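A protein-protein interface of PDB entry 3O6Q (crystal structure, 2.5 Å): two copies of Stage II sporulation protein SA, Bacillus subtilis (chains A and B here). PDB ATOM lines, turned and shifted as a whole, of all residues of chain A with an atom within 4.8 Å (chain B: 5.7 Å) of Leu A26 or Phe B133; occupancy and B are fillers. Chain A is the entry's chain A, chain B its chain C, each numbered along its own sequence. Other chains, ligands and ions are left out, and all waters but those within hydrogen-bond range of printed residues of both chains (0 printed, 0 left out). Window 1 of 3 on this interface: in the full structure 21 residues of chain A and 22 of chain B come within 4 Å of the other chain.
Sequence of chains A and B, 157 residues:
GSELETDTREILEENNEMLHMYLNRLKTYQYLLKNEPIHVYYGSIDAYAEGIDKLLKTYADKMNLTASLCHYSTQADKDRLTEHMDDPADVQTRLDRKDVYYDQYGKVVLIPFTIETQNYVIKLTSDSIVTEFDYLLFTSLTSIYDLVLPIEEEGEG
Positions printed for both chains: 22, 26 and 137.
Of the 11 pairs that touch across the chains among the printed residues, none has its exchanged pair printed and touching as well.
OE2 of Glu B132 lies within hydrogen-bond range of OG1 of Thr B131 (3.4 Å).
The side-chain hydroxyl (OG1) of Thr B131 is in hydrogen-bond range of the backbone NH (N) of Phe B133 (3.1 Å).
The backbone carbonyl oxygen of Leu B136 sits at hydrogen-bond distance from the side-chain hydroxyl of Ser B140 (2.6 Å).
Printed residues of chain B that touch a printed residue of chain A: Met B18, Glu B132, Phe B133, Tyr B135, Leu B136 and Ser B140.
Hydrophobic or aromatic side chains of chain B within 4 Å of the printed part of chain A: Met B18, Phe B133, Tyr B135 and Leu B136.
Of the 11 printed residues of chain A, 6 touch a printed residue of chain B.
Printed residues of chain A that touch a printed residue of chain B: Leu A19, Leu A23, Leu A26, Lys A27, Tyr A29 and Gln A30.
Hydrophobic or aromatic side chains of chain A that line the printed part of chain B: Leu A19, Leu A23, Leu A26 and Tyr A29.
Printed residues of chain B within 4 Å of Leu A19: Met B18 (3.6 Å).
Printed residues of chain B within 4 Å of Leu A23: Glu B132 (3.8 Å), Phe B133 (3.7 Å) and Leu B136 (3.9 Å).
Of chain B, only Phe B133 (3.7 Å) and Leu B136 (3.6 Å) come within 4 Å of Leu A26.
Of the printed residues of chain B, Tyr A29 touches Ser B140 (3.7 Å).
Of the printed residues of chain A, Phe B133 touches Leu A23 (3.7 Å) and Leu A26 (3.7 Å).
Of the printed residues of chain A, Ser B140 touches Tyr A29 and Gln A30.
The nearest printed residue of chain A that does not touch Phe B133 is Leu A19 (4.003 Å).
OE1 of Gln A30 sits at hydrogen-bond distance from OH of Tyr B135.
Met B18 touches Leu A19 (CB to CD2, 3.6 Å).
CD1 of Leu A23 touches CG of Glu B132, 3.8 Å away.
Leu A23 touches Phe B133 (CB to CZ, 3.7 Å).
Leu A23 touches Leu B136.
Phe B133 touches Leu A26.
CD2 of Leu A26 touches CB of Leu B136, at 3.6 Å.
CD1 of Leu B136 touches N of Lys A27, at 3.8 Å.
Tyr A29 touches Ser B140.
CB of Gln A30 touches CD2 of Leu B136, 3.5 Å away.
Gln A30 touches Ser B140.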
ATOM      1  N   LEU A  19     -33.438 -28.609 -11.772  1.00  0.00           N
ATOM      2  CA  LEU A  19     -33.826 -27.407 -11.035  1.00  0.00           C
ATOM      3  C   LEU A  19     -33.327 -27.452  -9.605  1.00  0.00           C
ATOM      4  O   LEU A  19     -32.897 -26.437  -9.068  1.00  0.00           O
ATOM      5  CB  LEU A  19     -35.340 -27.235 -11.012  1.00  0.00           C
ATOM      6  CG  LEU A  19     -36.000 -26.696 -12.301  1.00  0.00           C
ATOM      7  CD1 LEU A  19     -37.514 -26.987 -12.358  1.00  0.00           C
ATOM      8  CD2 LEU A  19     -35.672 -25.185 -12.496  1.00  0.00           C
ATOM      9  N   TYR A  22     -29.194 -27.151  -9.705  1.00  0.00           N
ATOM     10  CA  TYR A  22     -28.642 -25.848  -9.965  1.00  0.00           C
ATOM     11  C   TYR A  22     -29.145 -24.795  -8.981  1.00  0.00           C
ATOM     12  O   TYR A  22     -28.457 -23.820  -8.728  1.00  0.00           O
ATOM     13  CB  TYR A  22     -28.802 -25.489 -11.442  1.00  0.00           C
ATOM     14  CG  TYR A  22     -27.857 -26.331 -12.296  1.00  0.00           C
ATOM     15  CD1 TYR A  22     -26.483 -26.183 -12.172  1.00  0.00           C
ATOM     16  CD2 TYR A  22     -28.341 -27.319 -13.161  1.00  0.00           C
ATOM     17  CE1 TYR A  22     -25.599 -26.980 -12.905  1.00  0.00           C
ATOM     18  CE2 TYR A  22     -27.463 -28.118 -13.907  1.00  0.00           C
ATOM     19  CZ  TYR A  22     -26.089 -27.945 -13.780  1.00  0.00           C
ATOM     20  OH  TYR A  22     -25.217 -28.723 -14.522  1.00  0.00           O
ATOM     21  N   LEU A  23     -30.309 -25.003  -8.370  1.00  0.00           N
ATOM     22  CA  LEU A  23     -30.662 -24.198  -7.212  1.00  0.00           C
ATOM     23  C   LEU A  23     -29.672 -24.446  -6.079  1.00  0.00           C
ATOM     24  O   LEU A  23     -29.181 -23.478  -5.477  1.00  0.00           O
ATOM     25  CB  LEU A  23     -32.082 -24.478  -6.753  1.00  0.00           C
ATOM     26  CG  LEU A  23     -32.541 -23.764  -5.457  1.00  0.00           C
ATOM     27  CD1 LEU A  23     -32.437 -22.284  -5.557  1.00  0.00           C
ATOM     28  CD2 LEU A  23     -33.947 -24.197  -5.101  1.00  0.00           C
ATOM     29  N   ASN A  24     -29.355 -25.715  -5.795  1.00  0.00           N
ATOM     30  CA  ASN A  24     -28.382 -26.044  -4.722  1.00  0.00           C
ATOM     31  C   ASN A  24     -26.982 -25.478  -5.003  1.00  0.00           C
ATOM     32  O   ASN A  24     -26.316 -24.897  -4.114  1.00  0.00           O
ATOM     33  CB  ASN A  24     -28.259 -27.554  -4.475  1.00  0.00           C
ATOM     34  CG  ASN A  24     -29.515 -28.172  -3.860  1.00  0.00           C
ATOM     35  OD1 ASN A  24     -30.359 -27.475  -3.288  1.00  0.00           O
ATOM     36  ND2 ASN A  24     -29.634 -29.508  -3.959  1.00  0.00           N
ATOM     37  N   ARG A  25     -26.523 -25.650  -6.227  1.00  0.00           N
ATOM     38  CA  ARG A  25     -25.174 -25.209  -6.569  1.00  0.00           C
ATOM     39  C   ARG A  25     -25.131 -23.684  -6.511  1.00  0.00           C
ATOM     40  O   ARG A  25     -24.142 -23.123  -6.089  1.00  0.00           O
ATOM     41  CB  ARG A  25     -24.756 -25.738  -7.936  1.00  0.00           C
ATOM     42  CG  ARG A  25     -24.504 -27.191  -7.949  1.00  0.00           C
ATOM     43  CD  ARG A  25     -23.974 -27.702  -9.281  1.00  0.00           C
ATOM     44  NE  ARG A  25     -23.706 -29.127  -9.232  1.00  0.00           N
ATOM     45  CZ  ARG A  25     -23.429 -29.887 -10.292  1.00  0.00           C
ATOM     46  NH1 ARG A  25     -23.406 -29.385 -11.532  1.00  0.00           N
ATOM     47  NH2 ARG A  25     -23.200 -31.184 -10.100  1.00  0.00           N
ATOM     48  N   LEU A  26     -26.228 -23.029  -6.883  1.00  0.00           N
ATOM     49  CA  LEU A  26     -26.270 -21.571  -6.857  1.00  0.00           C
ATOM     50  C   LEU A  26     -26.381 -21.058  -5.409  1.00  0.00           C
ATOM     51  O   LEU A  26     -25.736 -20.084  -5.046  1.00  0.00           O
ATOM     52  CB  LEU A  26     -27.376 -21.027  -7.775  1.00  0.00           C
ATOM     53  CG  LEU A  26     -27.330 -19.486  -7.898  1.00  0.00           C
ATOM     54  CD1 LEU A  26     -25.973 -18.965  -8.445  1.00  0.00           C
ATOM     55  CD2 LEU A  26     -28.523 -18.977  -8.719  1.00  0.00           C
ATOM     56  N   LYS A  27     -27.140 -21.761  -4.569  1.00  0.00           N
ATOM     57  CA  LYS A  27     -27.116 -21.516  -3.118  1.00  0.00           C
ATOM     58  C   LYS A  27     -25.716 -21.596  -2.519  1.00  0.00           C
ATOM     59  O   LYS A  27     -25.289 -20.733  -1.767  1.00  0.00           O
ATOM     60  CB  LYS A  27     -28.010 -22.528  -2.390  1.00  0.00           C
ATOM     61  CG  LYS A  27     -29.488 -22.211  -2.481  1.00  0.00           C
ATOM     62  CD  LYS A  27     -30.340 -23.337  -2.012  1.00  0.00           C
ATOM     63  CE  LYS A  27     -30.274 -23.493  -0.507  1.00  0.00           C
ATOM     64  NZ  LYS A  27     -31.214 -24.597  -0.143  1.00  0.00           N
ATOM     65  N   THR A  28     -24.996 -22.646  -2.837  1.00  0.00           N
ATOM     66  CA  THR A  28     -23.609 -22.762  -2.400  1.00  0.00           C
ATOM     67  C   THR A  28     -22.723 -21.648  -2.888  1.00  0.00           C
ATOM     68  O   THR A  28     -21.937 -21.112  -2.129  1.00  0.00           O
ATOM     69  CB  THR A  28     -23.042 -24.103  -2.813  1.00  0.00           C
ATOM     70  OG1 THR A  28     -23.861 -25.113  -2.191  1.00  0.00           O
ATOM     71  CG2 THR A  28     -21.564 -24.299  -2.373  1.00  0.00           C
ATOM     72  N   TYR A  29     -22.830 -21.313  -4.171  1.00  0.00           N
ATOM     73  CA  TYR A  29     -21.995 -20.266  -4.782  1.00  0.00           C
ATOM     74  C   TYR A  29     -22.196 -18.938  -4.034  1.00  0.00           C
ATOM     75  O   TYR A  29     -21.242 -18.279  -3.637  1.00  0.00           O
ATOM     76  CB  TYR A  29     -22.368 -20.172  -6.268  1.00  0.00           C
ATOM     77  CG  TYR A  29     -21.862 -18.992  -7.082  1.00  0.00           C
ATOM     78  CD1 TYR A  29     -20.696 -19.070  -7.835  1.00  0.00           C
ATOM     79  CD2 TYR A  29     -22.629 -17.845  -7.208  1.00  0.00           C
ATOM     80  CE1 TYR A  29     -20.265 -17.995  -8.652  1.00  0.00           C
ATOM     81  CE2 TYR A  29     -22.216 -16.773  -8.032  1.00  0.00           C
ATOM     82  CZ  TYR A  29     -21.031 -16.853  -8.720  1.00  0.00           C
ATOM     83  OH  TYR A  29     -20.606 -15.780  -9.469  1.00  0.00           O
ATOM     84  N   GLN A  30     -23.450 -18.573  -3.824  1.00  0.00           N
ATOM     85  CA  GLN A  30     -23.780 -17.329  -3.169  1.00  0.00           C
ATOM     86  C   GLN A  30     -23.326 -17.366  -1.724  1.00  0.00           C
ATOM     87  O   GLN A  30     -22.829 -16.379  -1.230  1.00  0.00           O
ATOM     88  CB  GLN A  30     -25.270 -17.079  -3.227  1.00  0.00           C
ATOM     89  CG  GLN A  30     -25.682 -15.721  -2.638  1.00  0.00           C
ATOM     90  CD  GLN A  30     -26.341 -15.783  -1.247  1.00  0.00           C
ATOM     91  OE1 GLN A  30     -27.191 -14.929  -0.915  1.00  0.00           O
ATOM     92  NE2 GLN A  30     -25.943 -16.768  -0.427  1.00  0.00           N
ATOM     93  N   LEU A 137     -21.081 -20.715 -14.074  1.00  0.00           N
ATOM     94  CA  LEU A 137     -20.663 -20.456 -12.707  1.00  0.00           C
ATOM     95  C   LEU A 137     -19.156 -20.445 -12.632  1.00  0.00           C
ATOM     96  O   LEU A 137     -18.554 -19.563 -12.021  1.00  0.00           O
ATOM     97  CB  LEU A 137     -21.207 -21.510 -11.751  1.00  0.00           C
ATOM     98  CG  LEU A 137     -22.694 -21.393 -11.434  1.00  0.00           C
ATOM     99  CD1 LEU A 137     -23.136 -22.641 -10.701  1.00  0.00           C
ATOM    100  CD2 LEU A 137     -22.976 -20.098 -10.646  1.00  0.00           C
ATOM    101  N   MET B  18     -38.886 -22.206 -16.154  1.00  0.00           N
ATOM    102  CA  MET B  18     -37.879 -22.023 -15.100  1.00  0.00           C
ATOM    103  C   MET B  18     -36.452 -22.249 -15.606  1.00  0.00           C
ATOM    104  O   MET B  18     -35.544 -21.507 -15.270  1.00  0.00           O
ATOM    105  CB  MET B  18     -38.118 -23.007 -13.962  1.00  0.00           C
ATOM    106  CG  MET B  18     -39.315 -22.701 -13.060  1.00  0.00           C
ATOM    107  SD  MET B  18     -38.841 -21.519 -11.557  1.00  0.00           S
ATOM    108  CE  MET B  18     -38.143 -22.993 -10.470  1.00  0.00           C
ATOM    109  N   TYR B  22     -33.752 -19.105 -16.050  1.00  0.00           N
ATOM    110  CA  TYR B  22     -32.603 -19.009 -15.215  1.00  0.00           C
ATOM    111  C   TYR B  22     -31.289 -19.395 -15.869  1.00  0.00           C
ATOM    112  O   TYR B  22     -30.239 -18.891 -15.503  1.00  0.00           O
ATOM    113  CB  TYR B  22     -32.892 -19.703 -13.899  1.00  0.00           C
ATOM    114  CG  TYR B  22     -33.943 -18.872 -13.145  1.00  0.00           C
ATOM    115  CD1 TYR B  22     -33.671 -17.539 -12.770  1.00  0.00           C
ATOM    116  CD2 TYR B  22     -35.212 -19.372 -12.870  1.00  0.00           C
ATOM    117  CE1 TYR B  22     -34.617 -16.748 -12.117  1.00  0.00           C
ATOM    118  CE2 TYR B  22     -36.182 -18.573 -12.223  1.00  0.00           C
ATOM    119  CZ  TYR B  22     -35.863 -17.265 -11.850  1.00  0.00           C
ATOM    120  OH  TYR B  22     -36.782 -16.472 -11.215  1.00  0.00           O
ATOM    121  N   LEU B  26     -28.613 -16.394 -15.894  1.00  0.00           N
ATOM    122  CA  LEU B  26     -27.269 -16.760 -15.512  1.00  0.00           C
ATOM    123  C   LEU B  26     -26.278 -16.452 -16.631  1.00  0.00           C
ATOM    124  O   LEU B  26     -25.151 -15.997 -16.368  1.00  0.00           O
ATOM    125  CB  LEU B  26     -27.231 -18.223 -15.035  1.00  0.00           C
ATOM    126  CG  LEU B  26     -25.868 -18.694 -14.472  1.00  0.00           C
ATOM    127  CD1 LEU B  26     -25.496 -17.895 -13.217  1.00  0.00           C
ATOM    128  CD2 LEU B  26     -25.829 -20.218 -14.256  1.00  0.00           C
ATOM    129  N   THR B 131     -37.744 -15.055  -8.681  1.00  0.00           N
ATOM    130  CA  THR B 131     -37.684 -16.117  -7.691  1.00  0.00           C
ATOM    131  C   THR B 131     -36.391 -15.999  -6.888  1.00  0.00           C
ATOM    132  O   THR B 131     -35.585 -15.081  -7.079  1.00  0.00           O
ATOM    133  CB  THR B 131     -37.672 -17.545  -8.334  1.00  0.00           C
ATOM    134  OG1 THR B 131     -36.390 -17.774  -8.940  1.00  0.00           O
ATOM    135  CG2 THR B 131     -38.852 -17.773  -9.336  1.00  0.00           C
ATOM    136  N   GLU B 132     -36.208 -16.929  -5.957  1.00  0.00           N
ATOM    137  CA  GLU B 132     -34.934 -17.079  -5.239  1.00  0.00           C
ATOM    138  C   GLU B 132     -33.671 -17.130  -6.107  1.00  0.00           C
ATOM    139  O   GLU B 132     -32.592 -16.757  -5.670  1.00  0.00           O
ATOM    140  CB  GLU B 132     -35.004 -18.296  -4.320  1.00  0.00           C
ATOM    141  CG  GLU B 132     -35.122 -19.652  -4.995  1.00  0.00           C
ATOM    142  CD  GLU B 132     -36.413 -19.870  -5.809  1.00  0.00           C
ATOM    143  OE1 GLU B 132     -37.526 -19.477  -5.368  1.00  0.00           O
ATOM    144  OE2 GLU B 132     -36.271 -20.443  -6.913  1.00  0.00           O
ATOM    145  N   PHE B 133     -33.785 -17.576  -7.339  1.00  0.00           N
ATOM    146  CA  PHE B 133     -32.638 -17.549  -8.224  1.00  0.00           C
ATOM    147  C   PHE B 133     -32.171 -16.129  -8.405  1.00  0.00           C
ATOM    148  O   PHE B 133     -30.971 -15.860  -8.416  1.00  0.00           O
ATOM    149  CB  PHE B 133     -33.020 -18.135  -9.587  1.00  0.00           C
ATOM    150  CG  PHE B 133     -32.978 -19.652  -9.653  1.00  0.00           C
ATOM    151  CD1 PHE B 133     -34.124 -20.416  -9.332  1.00  0.00           C
ATOM    152  CD2 PHE B 133     -31.778 -20.311 -10.017  1.00  0.00           C
ATOM    153  CE1 PHE B 133     -34.115 -21.846  -9.399  1.00  0.00           C
ATOM    154  CE2 PHE B 133     -31.715 -21.704 -10.057  1.00  0.00           C
ATOM    155  CZ  PHE B 133     -32.920 -22.497  -9.774  1.00  0.00           C
ATOM    156  N   ASP B 134     -33.126 -15.210  -8.522  1.00  0.00           N
ATOM    157  CA  ASP B 134     -32.801 -13.775  -8.656  1.00  0.00           C
ATOM    158  C   ASP B 134     -32.232 -13.209  -7.374  1.00  0.00           C
ATOM    159  O   ASP B 134     -31.243 -12.482  -7.394  1.00  0.00           O
ATOM    160  CB  ASP B 134     -34.016 -12.987  -9.094  1.00  0.00           C
ATOM    161  CG  ASP B 134     -34.644 -13.562 -10.356  1.00  0.00           C
ATOM    162  OD1 ASP B 134     -33.967 -13.551 -11.393  1.00  0.00           O
ATOM    163  OD2 ASP B 134     -35.779 -14.080 -10.311  1.00  0.00           O
ATOM    164  N   TYR B 135     -32.805 -13.610  -6.258  1.00  0.00           N
ATOM    165  CA  TYR B 135     -32.197 -13.361  -4.965  1.00  0.00           C
ATOM    166  C   TYR B 135     -30.723 -13.764  -4.996  1.00  0.00           C
ATOM    167  O   TYR B 135     -29.831 -12.964  -4.688  1.00  0.00           O
ATOM    168  CB  TYR B 135     -32.931 -14.154  -3.885  1.00  0.00           C
ATOM    169  CG  TYR B 135     -32.177 -14.236  -2.608  1.00  0.00           C
ATOM    170  CD1 TYR B 135     -32.118 -13.161  -1.751  1.00  0.00           C
ATOM    171  CD2 TYR B 135     -31.480 -15.371  -2.270  1.00  0.00           C
ATOM    172  CE1 TYR B 135     -31.378 -13.228  -0.568  1.00  0.00           C
ATOM    173  CE2 TYR B 135     -30.740 -15.441  -1.107  1.00  0.00           C
ATOM    174  CZ  TYR B 135     -30.692 -14.372  -0.256  1.00  0.00           C
ATOM    175  OH  TYR B 135     -29.955 -14.463   0.921  1.00  0.00           O
ATOM    176  N   LEU B 136     -30.447 -15.004  -5.410  1.00  0.00           N
ATOM    177  CA  LEU B 136     -29.076 -15.488  -5.392  1.00  0.00           C
ATOM    178  C   LEU B 136     -28.187 -14.689  -6.311  1.00  0.00           C
ATOM    179  O   LEU B 136     -27.064 -14.332  -5.944  1.00  0.00           O
ATOM    180  CB  LEU B 136     -29.031 -16.951  -5.742  1.00  0.00           C
ATOM    181  CG  LEU B 136     -29.637 -17.881  -4.706  1.00  0.00           C
ATOM    182  CD1 LEU B 136     -29.924 -19.258  -5.302  1.00  0.00           C
ATOM    183  CD2 LEU B 136     -28.665 -17.982  -3.396  1.00  0.00           C
ATOM    184  N   LEU B 137     -28.663 -14.396  -7.522  1.00  0.00           N
ATOM    185  CA  LEU B 137     -27.815 -13.683  -8.482  1.00  0.00           C
ATOM    186  C   LEU B 137     -27.573 -12.268  -8.022  1.00  0.00           C
ATOM    187  O   LEU B 137     -26.435 -11.775  -8.040  1.00  0.00           O
ATOM    188  CB  LEU B 137     -28.441 -13.674  -9.880  1.00  0.00           C
ATOM    189  CG  LEU B 137     -28.289 -15.008 -10.617  1.00  0.00           C
ATOM    190  CD1 LEU B 137     -28.772 -14.856 -11.998  1.00  0.00           C
ATOM    191  CD2 LEU B 137     -26.857 -15.543 -10.682  1.00  0.00           C
ATOM    192  N   PHE B 138     -28.640 -11.589  -7.626  1.00  0.00           N
ATOM    193  CA  PHE B 138     -28.458 -10.208  -7.271  1.00  0.00           C
ATOM    194  C   PHE B 138     -27.711 -10.035  -5.984  1.00  0.00           C
ATOM    195  O   PHE B 138     -26.936  -9.095  -5.899  1.00  0.00           O
ATOM    196  CB  PHE B 138     -29.760  -9.422  -7.334  1.00  0.00           C
ATOM    197  CG  PHE B 138     -30.143  -9.048  -8.770  1.00  0.00           C
ATOM    198  CD1 PHE B 138     -29.747  -7.833  -9.320  1.00  0.00           C
ATOM    199  CD2 PHE B 138     -30.805  -9.971  -9.579  1.00  0.00           C
ATOM    200  CE1 PHE B 138     -30.072  -7.530 -10.639  1.00  0.00           C
ATOM    201  CE2 PHE B 138     -31.109  -9.687 -10.861  1.00  0.00           C
ATOM    202  CZ  PHE B 138     -30.755  -8.477 -11.408  1.00  0.00           C
ATOM    203  N   SER B 140     -25.373 -12.126  -4.875  1.00  0.00           N
ATOM    204  CA  SER B 140     -23.994 -12.411  -5.319  1.00  0.00           C
ATOM    205  C   SER B 140     -23.274 -11.171  -5.817  1.00  0.00           C
ATOM    206  O   SER B 140     -22.126 -10.956  -5.522  1.00  0.00           O
ATOM    207  CB  SER B 140     -24.027 -13.442  -6.452  1.00  0.00           C
ATOM    208  OG  SER B 140     -24.446 -14.702  -5.929  1.00  0.00           O
